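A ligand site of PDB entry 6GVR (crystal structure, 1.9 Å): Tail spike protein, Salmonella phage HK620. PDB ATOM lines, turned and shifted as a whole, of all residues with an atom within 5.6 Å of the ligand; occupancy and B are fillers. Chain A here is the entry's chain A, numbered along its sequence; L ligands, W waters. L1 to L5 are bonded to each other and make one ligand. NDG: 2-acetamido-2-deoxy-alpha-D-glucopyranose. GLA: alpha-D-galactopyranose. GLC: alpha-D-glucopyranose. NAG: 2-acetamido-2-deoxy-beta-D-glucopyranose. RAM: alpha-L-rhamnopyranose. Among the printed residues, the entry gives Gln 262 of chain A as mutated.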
ATOM      1  N   GLY A 101     -21.198  34.871 -22.753  1.00  0.00           N
ATOM      2  CA  GLY A 101     -21.463  33.432 -22.685  1.00  0.00           C
ATOM      3  C   GLY A 101     -20.328  32.605 -22.082  1.00  0.00           C
ATOM      4  O   GLY A 101     -20.520  31.421 -21.774  1.00  0.00           O
ATOM      5  N   HIS A 102     -19.134  33.203 -21.921  1.00  0.00           N
ATOM      6  CA  HIS A 102     -18.025  32.588 -21.273  1.00  0.00           C
ATOM      7  C   HIS A 102     -17.790  33.174 -19.893  1.00  0.00           C
ATOM      8  O   HIS A 102     -16.668  32.998 -19.328  1.00  0.00           O
ATOM      9  CB  HIS A 102     -16.752  32.803 -22.106  1.00  0.00           C
ATOM     10  CG  HIS A 102     -16.864  32.377 -23.507  1.00  0.00           C
ATOM     11  ND1 HIS A 102     -16.482  31.136 -23.952  1.00  0.00           N
ATOM     12  CD2 HIS A 102     -17.265  33.052 -24.607  1.00  0.00           C
ATOM     13  CE1 HIS A 102     -16.661  31.039 -25.244  1.00  0.00           C
ATOM     14  NE2 HIS A 102     -17.143  32.202 -25.674  1.00  0.00           N
ATOM     15  N   SER A 103     -18.788  33.886 -19.343  1.00  0.00           N
ATOM     16  CA  SER A 103     -18.653  34.659 -18.069  1.00  0.00           C
ATOM     17  C   SER A 103     -17.436  35.579 -18.108  1.00  0.00           C
ATOM     18  O   SER A 103     -16.780  35.767 -17.061  1.00  0.00           O
ATOM     19  CB  SER A 103     -18.526  33.683 -16.875  1.00  0.00           C
ATOM     20  OG  SER A 103     -19.691  32.897 -16.830  1.00  0.00           O
ATOM     21  N   GLN A 132     -14.201  34.382 -16.129  1.00  0.00           N
ATOM     22  CA  GLN A 132     -13.020  34.125 -16.964  1.00  0.00           C
ATOM     23  C   GLN A 132     -12.433  35.489 -17.254  1.00  0.00           C
ATOM     24  O   GLN A 132     -13.071  36.322 -17.863  1.00  0.00           O
ATOM     25  CB  GLN A 132     -13.399  33.341 -18.224  1.00  0.00           C
ATOM     26  CG  GLN A 132     -13.835  31.898 -17.924  1.00  0.00           C
ATOM     27  CD  GLN A 132     -13.854  31.049 -19.186  1.00  0.00           C
ATOM     28  OE1 GLN A 132     -12.802  30.795 -19.815  1.00  0.00           O
ATOM     29  NE2 GLN A 132     -15.044  30.533 -19.552  1.00  0.00           N
ATOM     30  N   PHE A 137     -12.218  34.578 -27.133  1.00  0.00           N
ATOM     31  CA  PHE A 137     -13.337  34.295 -28.046  1.00  0.00           C
ATOM     32  C   PHE A 137     -14.055  35.590 -28.313  1.00  0.00           C
ATOM     33  O   PHE A 137     -14.032  36.520 -27.480  1.00  0.00           O
ATOM     34  CB  PHE A 137     -14.313  33.258 -27.522  1.00  0.00           C
ATOM     35  CG  PHE A 137     -13.705  31.880 -27.216  1.00  0.00           C
ATOM     36  CD1 PHE A 137     -13.415  30.969 -28.216  1.00  0.00           C
ATOM     37  CD2 PHE A 137     -13.461  31.520 -25.909  1.00  0.00           C
ATOM     38  CE1 PHE A 137     -12.923  29.700 -27.873  1.00  0.00           C
ATOM     39  CE2 PHE A 137     -12.982  30.280 -25.554  1.00  0.00           C
ATOM     40  CZ  PHE A 137     -12.746  29.369 -26.524  1.00  0.00           C
ATOM     41  N   PRO A 142     -18.074  28.980 -29.285  1.00  0.00           N
ATOM     42  CA  PRO A 142     -16.707  28.912 -29.848  1.00  0.00           C
ATOM     43  C   PRO A 142     -16.586  28.432 -31.293  1.00  0.00           C
ATOM     44  O   PRO A 142     -15.699  28.882 -32.073  1.00  0.00           O
ATOM     45  CB  PRO A 142     -15.945  28.013 -28.858  1.00  0.00           C
ATOM     46  CG  PRO A 142     -16.878  27.672 -27.744  1.00  0.00           C
ATOM     47  CD  PRO A 142     -18.205  28.334 -27.968  1.00  0.00           C
ATOM     48  N   LEU A 172     -17.522  27.421 -13.626  1.00  0.00           N
ATOM     49  CA  LEU A 172     -16.140  27.480 -14.167  1.00  0.00           C
ATOM     50  C   LEU A 172     -15.507  28.823 -13.862  1.00  0.00           C
ATOM     51  O   LEU A 172     -16.175  29.878 -13.836  1.00  0.00           O
ATOM     52  CB  LEU A 172     -16.119  27.263 -15.654  1.00  0.00           C
ATOM     53  CG  LEU A 172     -16.736  25.966 -16.122  1.00  0.00           C
ATOM     54  CD1 LEU A 172     -16.954  26.085 -17.631  1.00  0.00           C
ATOM     55  CD2 LEU A 172     -15.943  24.725 -15.718  1.00  0.00           C
ATOM     56  N   ASN A 174     -11.639  30.870 -14.839  1.00  0.00           N
ATOM     57  CA  ASN A 174     -10.376  30.909 -15.646  1.00  0.00           C
ATOM     58  C   ASN A 174      -9.694  32.280 -15.425  1.00  0.00           C
ATOM     59  O   ASN A 174     -10.331  33.301 -15.192  1.00  0.00           O
ATOM     60  CB  ASN A 174     -10.702  30.646 -17.153  1.00  0.00           C
ATOM     61  CG  ASN A 174      -9.474  30.216 -17.982  1.00  0.00           C
ATOM     62  OD1 ASN A 174      -8.338  30.102 -17.462  1.00  0.00           O
ATOM     63  ND2 ASN A 174      -9.688  29.936 -19.291  1.00  0.00           N
ATOM     64  N   THR A 197     -10.873  26.871 -12.003  1.00  0.00           N
ATOM     65  CA  THR A 197     -10.860  25.626 -12.733  1.00  0.00           C
ATOM     66  C   THR A 197      -9.487  25.559 -13.479  1.00  0.00           C
ATOM     67  O   THR A 197      -8.815  24.538 -13.478  1.00  0.00           O
ATOM     68  CB  THR A 197     -11.951  25.600 -13.753  1.00  0.00           C
ATOM     69  OG1 THR A 197     -13.237  25.833 -13.124  1.00  0.00           O
ATOM     70  CG2 THR A 197     -11.963  24.308 -14.489  1.00  0.00           C
ATOM     71  N   TRP A 198      -9.149  26.658 -14.074  1.00  0.00           N
ATOM     72  CA  TRP A 198      -7.858  26.873 -14.774  1.00  0.00           C
ATOM     73  C   TRP A 198      -7.324  28.274 -14.526  1.00  0.00           C
ATOM     74  O   TRP A 198      -8.093  29.190 -14.180  1.00  0.00           O
ATOM     75  CB  TRP A 198      -8.010  26.751 -16.265  1.00  0.00           C
ATOM     76  CG  TRP A 198      -8.843  25.588 -16.801  1.00  0.00           C
ATOM     77  CD1 TRP A 198      -8.496  24.286 -16.884  1.00  0.00           C
ATOM     78  CD2 TRP A 198     -10.204  25.675 -17.270  1.00  0.00           C
ATOM     79  NE1 TRP A 198      -9.516  23.552 -17.431  1.00  0.00           N
ATOM     80  CE2 TRP A 198     -10.587  24.401 -17.685  1.00  0.00           C
ATOM     81  CE3 TRP A 198     -11.102  26.740 -17.443  1.00  0.00           C
ATOM     82  CZ2 TRP A 198     -11.832  24.142 -18.203  1.00  0.00           C
ATOM     83  CZ3 TRP A 198     -12.397  26.453 -17.908  1.00  0.00           C
ATOM     84  CH2 TRP A 198     -12.717  25.182 -18.324  1.00  0.00           C
ATOM     85  N   THR A 201      -5.966  28.836 -20.438  1.00  0.00           N
ATOM     86  CA  THR A 201      -6.252  27.819 -21.434  1.00  0.00           C
ATOM     87  C   THR A 201      -5.820  28.314 -22.785  1.00  0.00           C
ATOM     88  O   THR A 201      -5.979  29.505 -23.065  1.00  0.00           O
ATOM     89  CB  THR A 201      -7.734  27.500 -21.518  1.00  0.00           C
ATOM     90  OG1 THR A 201      -8.491  28.634 -21.942  1.00  0.00           O
ATOM     91  CG2 THR A 201      -8.255  27.025 -20.191  1.00  0.00           C
ATOM     92  N   LEU A 202      -5.315  27.407 -23.616  1.00  0.00           N
ATOM     93  CA  LEU A 202      -4.707  27.760 -24.893  1.00  0.00           C
ATOM     94  C   LEU A 202      -5.461  26.996 -25.959  1.00  0.00           C
ATOM     95  O   LEU A 202      -5.702  25.812 -25.837  1.00  0.00           O
ATOM     96  CB  LEU A 202      -3.256  27.388 -24.965  1.00  0.00           C
ATOM     97  CG  LEU A 202      -2.334  27.821 -23.862  1.00  0.00           C
ATOM     98  CD1 LEU A 202      -0.911  27.304 -24.226  1.00  0.00           C
ATOM     99  CD2 LEU A 202      -2.364  29.305 -23.596  1.00  0.00           C
ATOM    100  N   GLY A 203      -5.879  27.671 -26.989  1.00  0.00           N
ATOM    101  CA  GLY A 203      -6.594  26.946 -28.041  1.00  0.00           C
ATOM    102  C   GLY A 203      -8.046  26.586 -27.671  1.00  0.00           C
ATOM    103  O   GLY A 203      -8.519  26.831 -26.498  1.00  0.00           O
ATOM    104  N   TRP A 204      -8.722  26.028 -28.652  1.00  0.00           N
ATOM    105  CA  TRP A 204     -10.112  25.477 -28.471  1.00  0.00           C
ATOM    106  C   TRP A 204     -10.243  24.313 -29.396  1.00  0.00           C
ATOM    107  O   TRP A 204     -10.213  24.511 -30.641  1.00  0.00           O
ATOM    108  CB  TRP A 204     -11.204  26.517 -28.711  1.00  0.00           C
ATOM    109  CG  TRP A 204     -12.551  25.888 -28.631  1.00  0.00           C
ATOM    110  CD1 TRP A 204     -13.154  25.425 -27.512  1.00  0.00           C
ATOM    111  CD2 TRP A 204     -13.410  25.508 -29.742  1.00  0.00           C
ATOM    112  NE1 TRP A 204     -14.383  24.832 -27.822  1.00  0.00           N
ATOM    113  CE2 TRP A 204     -14.546  24.838 -29.187  1.00  0.00           C
ATOM    114  CE3 TRP A 204     -13.345  25.676 -31.112  1.00  0.00           C
ATOM    115  CZ2 TRP A 204     -15.569  24.348 -29.957  1.00  0.00           C
ATOM    116  CZ3 TRP A 204     -14.354  25.188 -31.899  1.00  0.00           C
ATOM    117  CH2 TRP A 204     -15.489  24.540 -31.304  1.00  0.00           C
ATOM    118  N   ASN A 205     -10.394  23.122 -28.813  1.00  0.00           N
ATOM    119  CA  ASN A 205     -10.592  21.881 -29.554  1.00  0.00           C
ATOM    120  C   ASN A 205      -9.745  21.745 -30.799  1.00  0.00           C
ATOM    121  O   ASN A 205     -10.196  21.414 -31.900  1.00  0.00           O
ATOM    122  CB  ASN A 205     -12.063  21.688 -29.830  1.00  0.00           C
ATOM    123  CG  ASN A 205     -12.877  21.463 -28.570  1.00  0.00           C
ATOM    124  OD1 ASN A 205     -12.364  21.493 -27.409  1.00  0.00           O
ATOM    125  ND2 ASN A 205     -14.196  21.420 -28.770  1.00  0.00           N
ATOM    126  N   ASP A 229     -12.689  20.522  -9.772  1.00  0.00           N
ATOM    127  CA  ASP A 229     -11.565  20.038 -10.590  1.00  0.00           C
ATOM    128  C   ASP A 229     -10.710  21.209 -10.992  1.00  0.00           C
ATOM    129  O   ASP A 229     -11.236  22.321 -11.249  1.00  0.00           O
ATOM    130  CB  ASP A 229     -12.125  19.358 -11.842  1.00  0.00           C
ATOM    131  CG  ASP A 229     -11.122  18.486 -12.523  1.00  0.00           C
ATOM    132  OD1 ASP A 229      -9.894  18.348 -12.086  1.00  0.00           O
ATOM    133  OD2 ASP A 229     -11.605  17.959 -13.523  1.00  0.00           O
ATOM    134  N   HIS A 230      -9.413  21.007 -11.063  1.00  0.00           N
ATOM    135  CA  HIS A 230      -8.532  22.072 -11.451  1.00  0.00           C
ATOM    136  C   HIS A 230      -7.371  21.543 -12.307  1.00  0.00           C
ATOM    137  O   HIS A 230      -6.769  20.543 -11.995  1.00  0.00           O
ATOM    138  CB  HIS A 230      -7.947  22.806 -10.246  1.00  0.00           C
ATOM    139  CG  HIS A 230      -6.887  23.799 -10.603  1.00  0.00           C
ATOM    140  ND1 HIS A 230      -7.121  25.170 -10.644  1.00  0.00           N
ATOM    141  CD2 HIS A 230      -5.573  23.621 -10.875  1.00  0.00           C
ATOM    142  CE1 HIS A 230      -5.979  25.762 -10.967  1.00  0.00           C
ATOM    143  NE2 HIS A 230      -5.034  24.844 -11.108  1.00  0.00           N
ATOM    144  N   SER A 231      -7.112  22.271 -13.392  1.00  0.00           N
ATOM    145  CA  SER A 231      -5.883  22.045 -14.227  1.00  0.00           C
ATOM    146  C   SER A 231      -5.332  23.422 -14.516  1.00  0.00           C
ATOM    147  O   SER A 231      -6.052  24.236 -15.126  1.00  0.00           O
ATOM    148  CB  SER A 231      -6.207  21.301 -15.522  1.00  0.00           C
ATOM    149  OG  SER A 231      -6.572  19.946 -15.216  1.00  0.00           O
ATOM    150  N   TYR A 234      -4.288  24.470 -19.600  1.00  0.00           N
ATOM    151  CA  TYR A 234      -4.900  23.480 -20.494  1.00  0.00           C
ATOM    152  C   TYR A 234      -4.465  23.829 -21.912  1.00  0.00           C
ATOM    153  O   TYR A 234      -4.787  24.908 -22.452  1.00  0.00           O
ATOM    154  CB  TYR A 234      -6.428  23.538 -20.418  1.00  0.00           C
ATOM    155  CG  TYR A 234      -7.227  22.325 -20.864  1.00  0.00           C
ATOM    156  CD1 TYR A 234      -7.322  21.978 -22.207  1.00  0.00           C
ATOM    157  CD2 TYR A 234      -7.940  21.530 -19.951  1.00  0.00           C
ATOM    158  CE1 TYR A 234      -8.082  20.878 -22.606  1.00  0.00           C
ATOM    159  CE2 TYR A 234      -8.705  20.450 -20.351  1.00  0.00           C
ATOM    160  CZ  TYR A 234      -8.834  20.156 -21.700  1.00  0.00           C
ATOM    161  OH  TYR A 234      -9.635  19.110 -22.092  1.00  0.00           O
ATOM    162  N   ASN A 236      -4.794  23.194 -25.594  1.00  0.00           N
ATOM    163  CA  ASN A 236      -5.794  22.598 -26.529  1.00  0.00           C
ATOM    164  C   ASN A 236      -5.636  23.101 -27.966  1.00  0.00           C
ATOM    165  O   ASN A 236      -6.543  23.073 -28.817  1.00  0.00           O
ATOM    166  CB  ASN A 236      -7.191  22.842 -26.012  1.00  0.00           C
ATOM    167  CG  ASN A 236      -8.197  21.780 -26.435  1.00  0.00           C
ATOM    168  OD1 ASN A 236      -7.854  20.768 -27.035  1.00  0.00           O
ATOM    169  ND2 ASN A 236      -9.535  22.056 -26.146  1.00  0.00           N
ATOM    170  N   GLN A 262      -2.470  20.225 -18.816  1.00  0.00           N
ATOM    171  CA  GLN A 262      -3.158  19.299 -19.734  1.00  0.00           C
ATOM    172  C   GLN A 262      -2.493  19.444 -21.112  1.00  0.00           C
ATOM    173  O   GLN A 262      -2.577  20.546 -21.642  1.00  0.00           O
ATOM    174  CB  GLN A 262      -4.691  19.643 -19.865  1.00  0.00           C
ATOM    175  CG  GLN A 262      -5.453  19.536 -18.522  1.00  0.00           C
ATOM    176  CD  GLN A 262      -5.770  18.099 -18.019  1.00  0.00           C
ATOM    177  OE1 GLN A 262      -5.854  17.890 -16.775  1.00  0.00           O
ATOM    178  NE2 GLN A 262      -6.010  17.138 -18.921  1.00  0.00           N
ATOM    179  N   HIS A 264      -3.194  18.319 -24.768  1.00  0.00           N
ATOM    180  CA  HIS A 264      -4.322  17.659 -25.415  1.00  0.00           C
ATOM    181  C   HIS A 264      -4.309  17.748 -26.907  1.00  0.00           C
ATOM    182  O   HIS A 264      -5.337  17.368 -27.518  1.00  0.00           O
ATOM    183  CB  HIS A 264      -5.633  18.208 -24.914  1.00  0.00           C
ATOM    184  CG  HIS A 264      -6.063  17.649 -23.619  1.00  0.00           C
ATOM    185  ND1 HIS A 264      -7.379  17.344 -23.347  1.00  0.00           N
ATOM    186  CD2 HIS A 264      -5.364  17.275 -22.525  1.00  0.00           C
ATOM    187  CE1 HIS A 264      -7.477  16.844 -22.125  1.00  0.00           C
ATOM    188  NE2 HIS A 264      -6.290  16.856 -21.575  1.00  0.00           N
ATOM    189  N   TYR A 283      -1.724  15.523 -17.571  1.00  0.00           N
ATOM    190  CA  TYR A 283      -2.433  14.575 -18.414  1.00  0.00           C
ATOM    191  C   TYR A 283      -1.944  14.760 -19.863  1.00  0.00           C
ATOM    192  O   TYR A 283      -1.773  15.892 -20.306  1.00  0.00           O
ATOM    193  CB  TYR A 283      -3.922  14.814 -18.397  1.00  0.00           C
ATOM    194  CG  TYR A 283      -4.650  14.372 -17.140  1.00  0.00           C
ATOM    195  CD1 TYR A 283      -4.691  15.201 -16.015  1.00  0.00           C
ATOM    196  CD2 TYR A 283      -5.360  13.142 -17.102  1.00  0.00           C
ATOM    197  CE1 TYR A 283      -5.468  14.845 -14.869  1.00  0.00           C
ATOM    198  CE2 TYR A 283      -6.063  12.764 -15.916  1.00  0.00           C
ATOM    199  CZ  TYR A 283      -6.096  13.613 -14.817  1.00  0.00           C
ATOM    200  OH  TYR A 283      -6.821  13.237 -13.688  1.00  0.00           O
ATOM    201  N   VAL A 285      -3.300  13.463 -23.297  1.00  0.00           N
ATOM    202  CA  VAL A 285      -4.599  12.814 -23.617  1.00  0.00           C
ATOM    203  C   VAL A 285      -5.069  13.285 -24.976  1.00  0.00           C
ATOM    204  O   VAL A 285      -5.057  14.507 -25.192  1.00  0.00           O
ATOM    205  CB  VAL A 285      -5.711  13.178 -22.574  1.00  0.00           C
ATOM    206  CG1 VAL A 285      -7.110  12.724 -23.055  1.00  0.00           C
ATOM    207  CG2 VAL A 285      -5.454  12.536 -21.235  1.00  0.00           C
ATOM    208  N   HIS A 287      -8.609  13.555 -26.555  1.00  0.00           N
ATOM    209  CA  HIS A 287     -10.072  13.386 -26.398  1.00  0.00           C
ATOM    210  C   HIS A 287     -10.697  13.472 -27.823  1.00  0.00           C
ATOM    211  O   HIS A 287     -10.618  14.500 -28.477  1.00  0.00           O
ATOM    212  CB  HIS A 287     -10.693  14.493 -25.563  1.00  0.00           C
ATOM    213  CG  HIS A 287     -10.528  14.393 -24.069  1.00  0.00           C
ATOM    214  ND1 HIS A 287     -10.780  13.247 -23.359  1.00  0.00           N
ATOM    215  CD2 HIS A 287     -10.370  15.378 -23.141  1.00  0.00           C
ATOM    216  CE1 HIS A 287     -10.639  13.489 -22.062  1.00  0.00           C
ATOM    217  NE2 HIS A 287     -10.354  14.770 -21.902  1.00  0.00           N
ATOM    218  N   ALA A 289     -13.591  14.186 -28.502  1.00  0.00           N
ATOM    219  CA  ALA A 289     -14.396  15.375 -28.479  1.00  0.00           C
ATOM    220  C   ALA A 289     -13.694  16.693 -28.749  1.00  0.00           C
ATOM    221  O   ALA A 289     -14.356  17.713 -29.011  1.00  0.00           O
ATOM    222  CB  ALA A 289     -15.184  15.445 -27.170  1.00  0.00           C
ATOM    223  N   GLU A 290     -12.369  16.717 -28.742  1.00  0.00           N
ATOM    224  CA  GLU A 290     -11.620  17.907 -28.928  1.00  0.00           C
ATOM    225  C   GLU A 290     -10.835  17.858 -30.206  1.00  0.00           C
ATOM    226  O   GLU A 290      -9.826  18.582 -30.380  1.00  0.00           O
ATOM    227  CB  GLU A 290     -10.610  18.058 -27.713  1.00  0.00           C
ATOM    228  CG  GLU A 290     -11.327  18.248 -26.382  1.00  0.00           C
ATOM    229  CD  GLU A 290     -10.376  18.465 -25.230  1.00  0.00           C
ATOM    230  OE1 GLU A 290      -9.265  17.855 -25.289  1.00  0.00           O
ATOM    231  OE2 GLU A 290     -10.780  19.174 -24.291  1.00  0.00           O
ATOM    232  N   PRO A 359      -7.649   7.762 -19.064  1.00  0.00           N
ATOM    233  CA  PRO A 359      -7.971   8.615 -17.863  1.00  0.00           C
ATOM    234  C   PRO A 359      -9.372   8.199 -17.215  1.00  0.00           C
ATOM    235  O   PRO A 359      -9.468   7.737 -16.051  1.00  0.00           O
ATOM    236  CB  PRO A 359      -8.036  10.044 -18.486  1.00  0.00           C
ATOM    237  CG  PRO A 359      -8.393   9.836 -19.989  1.00  0.00           C
ATOM    238  CD  PRO A 359      -8.313   8.331 -20.281  1.00  0.00           C
HETATM  239  C1  NDG L   1      -8.758  16.751 -16.194  1.00  0.00           C
HETATM  240  C2  NDG L   1      -9.582  17.823 -16.939  1.00  0.00           C
HETATM  241  C3  NDG L   1     -10.722  17.152 -17.741  1.00  0.00           C
HETATM  242  C4  NDG L   1     -10.112  16.089 -18.664  1.00  0.00           C
HETATM  243  C5  NDG L   1      -9.275  15.075 -17.856  1.00  0.00           C
HETATM  244  C6  NDG L   1      -8.504  14.084 -18.663  1.00  0.00           C
HETATM  245  C7  NDG L   1      -9.823  20.142 -16.076  1.00  0.00           C
HETATM  246  C8  NDG L   1     -10.272  20.975 -14.934  1.00  0.00           C
HETATM  247  O5  NDG L   1      -8.291  15.740 -17.095  1.00  0.00           O
HETATM  248  O3  NDG L   1     -11.380  18.175 -18.560  1.00  0.00           O
HETATM  249  O4  NDG L   1     -11.063  15.416 -19.511  1.00  0.00           O
HETATM  250  O6  NDG L   1      -7.546  14.902 -19.378  1.00  0.00           O
HETATM  251  O7  NDG L   1      -9.319  20.661 -17.081  1.00  0.00           O
HETATM  252  N2  NDG L   1     -10.041  18.808 -15.974  1.00  0.00           N
HETATM  253  O1  NDG L   1      -9.571  16.088 -15.274  1.00  0.00           O
HETATM  254  C1  GLA L   2     -12.776  17.950 -18.772  1.00  0.00           C
HETATM  255  C2  GLA L   2     -13.124  18.710 -20.031  1.00  0.00           C
HETATM  256  C3  GLA L   2     -12.964  20.240 -19.869  1.00  0.00           C
HETATM  257  C4  GLA L   2     -13.649  20.721 -18.588  1.00  0.00           C
HETATM  258  C5  GLA L   2     -13.187  19.870 -17.390  1.00  0.00           C
HETATM  259  C6  GLA L   2     -13.841  20.186 -16.055  1.00  0.00           C
HETATM  260  O2  GLA L   2     -12.282  18.253 -21.115  1.00  0.00           O
HETATM  261  O3  GLA L   2     -13.532  20.833 -21.049  1.00  0.00           O
HETATM  262  O4  GLA L   2     -15.087  20.562 -18.730  1.00  0.00           O
HETATM  263  O5  GLA L   2     -13.409  18.474 -17.675  1.00  0.00           O
HETATM  264  O6  GLA L   2     -13.662  21.571 -15.807  1.00  0.00           O
HETATM  265  C1  GLC L   3     -15.794  21.772 -18.326  1.00  0.00           C
HETATM  266  C2  GLC L   3     -17.313  21.474 -18.240  1.00  0.00           C
HETATM  267  C3  GLC L   3     -17.921  21.076 -19.586  1.00  0.00           C
HETATM  268  C4  GLC L   3     -17.634  22.208 -20.499  1.00  0.00           C
HETATM  269  C5  GLC L   3     -16.128  22.461 -20.585  1.00  0.00           C
HETATM  270  C6  GLC L   3     -15.762  23.609 -21.538  1.00  0.00           C
HETATM  271  O2  GLC L   3     -17.531  20.469 -17.337  1.00  0.00           O
HETATM  272  O3  GLC L   3     -19.324  21.003 -19.421  1.00  0.00           O
HETATM  273  O4  GLC L   3     -18.228  21.941 -21.739  1.00  0.00           O
HETATM  274  O5  GLC L   3     -15.617  22.807 -19.262  1.00  0.00           O
HETATM  275  O6  GLC L   3     -16.351  24.885 -21.132  1.00  0.00           O
HETATM  276  C1  NAG L   4     -12.543  21.446 -21.876  1.00  0.00           C
HETATM  277  C2  NAG L   4     -13.128  21.604 -23.271  1.00  0.00           C
HETATM  278  C3  NAG L   4     -12.198  22.364 -24.203  1.00  0.00           C
HETATM  279  C4  NAG L   4     -11.615  23.590 -23.576  1.00  0.00           C
HETATM  280  C5  NAG L   4     -11.043  23.180 -22.261  1.00  0.00           C
HETATM  281  C6  NAG L   4     -10.317  24.315 -21.619  1.00  0.00           C
HETATM  282  C7  NAG L   4     -14.613  19.872 -24.101  1.00  0.00           C
HETATM  283  C8  NAG L   4     -14.793  18.444 -24.578  1.00  0.00           C
HETATM  284  N2  NAG L   4     -13.381  20.282 -23.768  1.00  0.00           N
HETATM  285  O3  NAG L   4     -12.990  22.738 -25.286  1.00  0.00           O
HETATM  286  O4  NAG L   4     -10.543  24.027 -24.419  1.00  0.00           O
HETATM  287  O5  NAG L   4     -12.093  22.709 -21.377  1.00  0.00           O
HETATM  288  O6  NAG L   4     -11.273  25.271 -21.286  1.00  0.00           O
HETATM  289  O7  NAG L   4     -15.559  20.639 -24.100  1.00  0.00           O
HETATM  290  C1  RAM L   5     -17.253  25.372 -22.158  1.00  0.00           C
HETATM  291  C2  RAM L   5     -18.065  26.518 -21.548  1.00  0.00           C
HETATM  292  C3  RAM L   5     -17.215  27.753 -21.273  1.00  0.00           C
HETATM  293  C4  RAM L   5     -16.388  28.084 -22.529  1.00  0.00           C
HETATM  294  C5  RAM L   5     -15.682  26.835 -23.099  1.00  0.00           C
HETATM  295  C6  RAM L   5     -14.941  27.071 -24.430  1.00  0.00           C
HETATM  296  O2  RAM L   5     -19.069  26.759 -22.517  1.00  0.00           O
HETATM  297  O3  RAM L   5     -18.059  28.853 -20.828  1.00  0.00           O
HETATM  298  O4  RAM L   5     -15.511  29.184 -22.225  1.00  0.00           O
HETATM  299  O5  RAM L   5     -16.603  25.769 -23.360  1.00  0.00           O
HETATM  300  O   HOH W   1     -12.869  13.838 -18.621  1.00  0.00           O
HETATM  301  O   HOH W   2     -18.690  21.664 -15.327  1.00  0.00           O
HETATM  302  O   HOH W   3     -10.967  26.624 -25.120  1.00  0.00           O
HETATM  303  O   HOH W   4     -20.490  24.477 -22.581  1.00  0.00           O
HETATM  304  O   HOH W   5     -14.786  21.834 -13.336  1.00  0.00           O
HETATM  305  O   HOH W   6     -18.144  29.982 -18.090  1.00  0.00           O
HETATM  306  O   HOH W   7     -13.755  16.053 -21.930  1.00  0.00           O
HETATM  307  O   HOH W   8     -16.388  17.900 -18.135  1.00  0.00           O
HETATM  308  O   HOH W   9     -16.195  21.410 -26.679  1.00  0.00           O
HETATM  309  O   HOH W  10     -20.689  28.726 -20.284  1.00  0.00           O
HETATM  310  O   HOH W  11     -19.610  29.369 -24.257  1.00  0.00           O
HETATM  311  O   HOH W  12     -15.698  23.792 -25.359  1.00  0.00           O
HETATM  312  O   HOH W  13     -20.902  19.938 -21.405  1.00  0.00           O
HETATM  313  O   HOH W  14     -12.885  29.637 -22.009  1.00  0.00           O
HETATM  314  O   HOH W  15     -11.028  27.743 -22.667  1.00  0.00           O
HETATM  315  O   HOH W  16      -8.776  15.217 -12.930  1.00  0.00           O
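The backbone NH (N) of Asn 205 lies close to the side-chain amide nitrogen (ND2) of Asn 236, at 3.0 Å. O of His 102 lies within hydrogen-bond range of NE2 of Gln 132. The backbone carbonyl oxygen (O) of Leu 202 is in hydrogen-bond range of the backbone NH (N) of Asn 236, at 2.8 Å. OE1 of Glu 290 lies within hydrogen-bond range of ND1 of His 264 (2.8 Å). The backbone carbonyl oxygen (O) of Trp 198 lies close to the side-chain amide oxygen (OD1) of Asn 174. N of Leu 202 lies within hydrogen-bond range of O of Tyr 234 (2.8 Å). O of Ser 103 is in hydrogen-bond range of N of Gln 132 (3.1 Å). OG1 of Thr 201 sits at hydrogen-bond distance from ND2 of Asn 174 (3.2 Å).
Water W16 lies within hydrogen-bond range of O1 of NDG L1, OH of Tyr 283 and OD1 of Asp 229. Water W14 bridges the side-chain amide oxygen of Gln 132 (2.5 Å) and an oxygen (O4) of RAM L5 (2.7 Å). Water W3 bridges O4 of NAG L4 (2.7 Å) and O of Gly 203 (2.8 Å). Water W9 lies within hydrogen-bond range of an oxygen (O7) of NAG L4 and the side-chain amide nitrogen (ND2) of Asn 205. Water W6 bridges O3 of RAM L5 and NE2 of Gln 132. Water W11 bridges an oxygen (O2) of RAM L5 (3.2 Å) and the backbone carbonyl oxygen (O) of Gly 101 (3.3 Å).
O3 of NAG L4 lies within hydrogen-bond range of OD1 of Asn 205 (2.5 Å). NE2 of His 287 is in hydrogen-bond range of O4 of NDG L1, 2.6 Å away. An oxygen (O6) of NDG L1 sits at hydrogen-bond distance from the side-chain amide nitrogen (NE2) of Gln 262 (2.8 Å). A ring nitrogen (ND1) of His 102 sits at hydrogen-bond distance from an oxygen (O4) of RAM L5 (2.8 Å). An oxygen (O4) of NAG L4 sits at hydrogen-bond distance from the side-chain amide nitrogen (ND2) of Asn 236 (2.8 Å). A nitrogen (N2) of NAG L4 is in hydrogen-bond range of the side-chain carboxylate (OE2) of Glu 290, 2.9 Å away. NE1 of Trp 198 sits at hydrogen-bond distance from O7 of NDG L1 (2.9 Å). An oxygen (O2) of GLA L2 lies within hydrogen-bond range of the side-chain hydroxyl (OH) of Tyr 234. The side-chain carboxylate (OD2) of Asp 229 sits at hydrogen-bond distance from a nitrogen (N2) of NDG L1 (3.0 Å). The side-chain amide nitrogen of Gln 132 sits at hydrogen-bond distance from an oxygen (O4) of RAM L5 (3.0 Å). NE2 of His 264 sits at hydrogen-bond distance from O6 of NDG L1, 3.2 Å away. The side-chain hydroxyl of Ser 231 sits close to an oxygen (O7) of NDG L1, at 3.4 Å.
O of Gly 101 touches O3 of RAM L5, at 3.7 Å. Phe 137 touches the ligand. Pro 142 touches the ligand. CD1 of Leu 172 touches O6 of GLC L3 (3.7 Å). Thr 197 touches the ligand. CG2 of Thr 201 touches O6 of NAG L4 (3.7 Å). Trp 204 touches the ligand. C of His 230 touches C8 of NDG L1, 3.95 Å away. CD2 of Tyr 283 touches O6 of NDG L1, 3.6 Å away. Val 285 touches the ligand. CB of Ala 289 touches C8 of NAG L4 (3.98 Å). Hydrophobic or aromatic side chains that line the ligand: His 102, Phe 137, Pro 142, Leu 172, Trp 198, Trp 204, Tyr 234, His 264, Tyr 283, Val 285, His 287 and Ala 289. Of the 28 residues printed, 23 come within 4 Å of the ligand. The nearest printed residue that does not touch the ligand is Gly 203 (4.04 Å).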
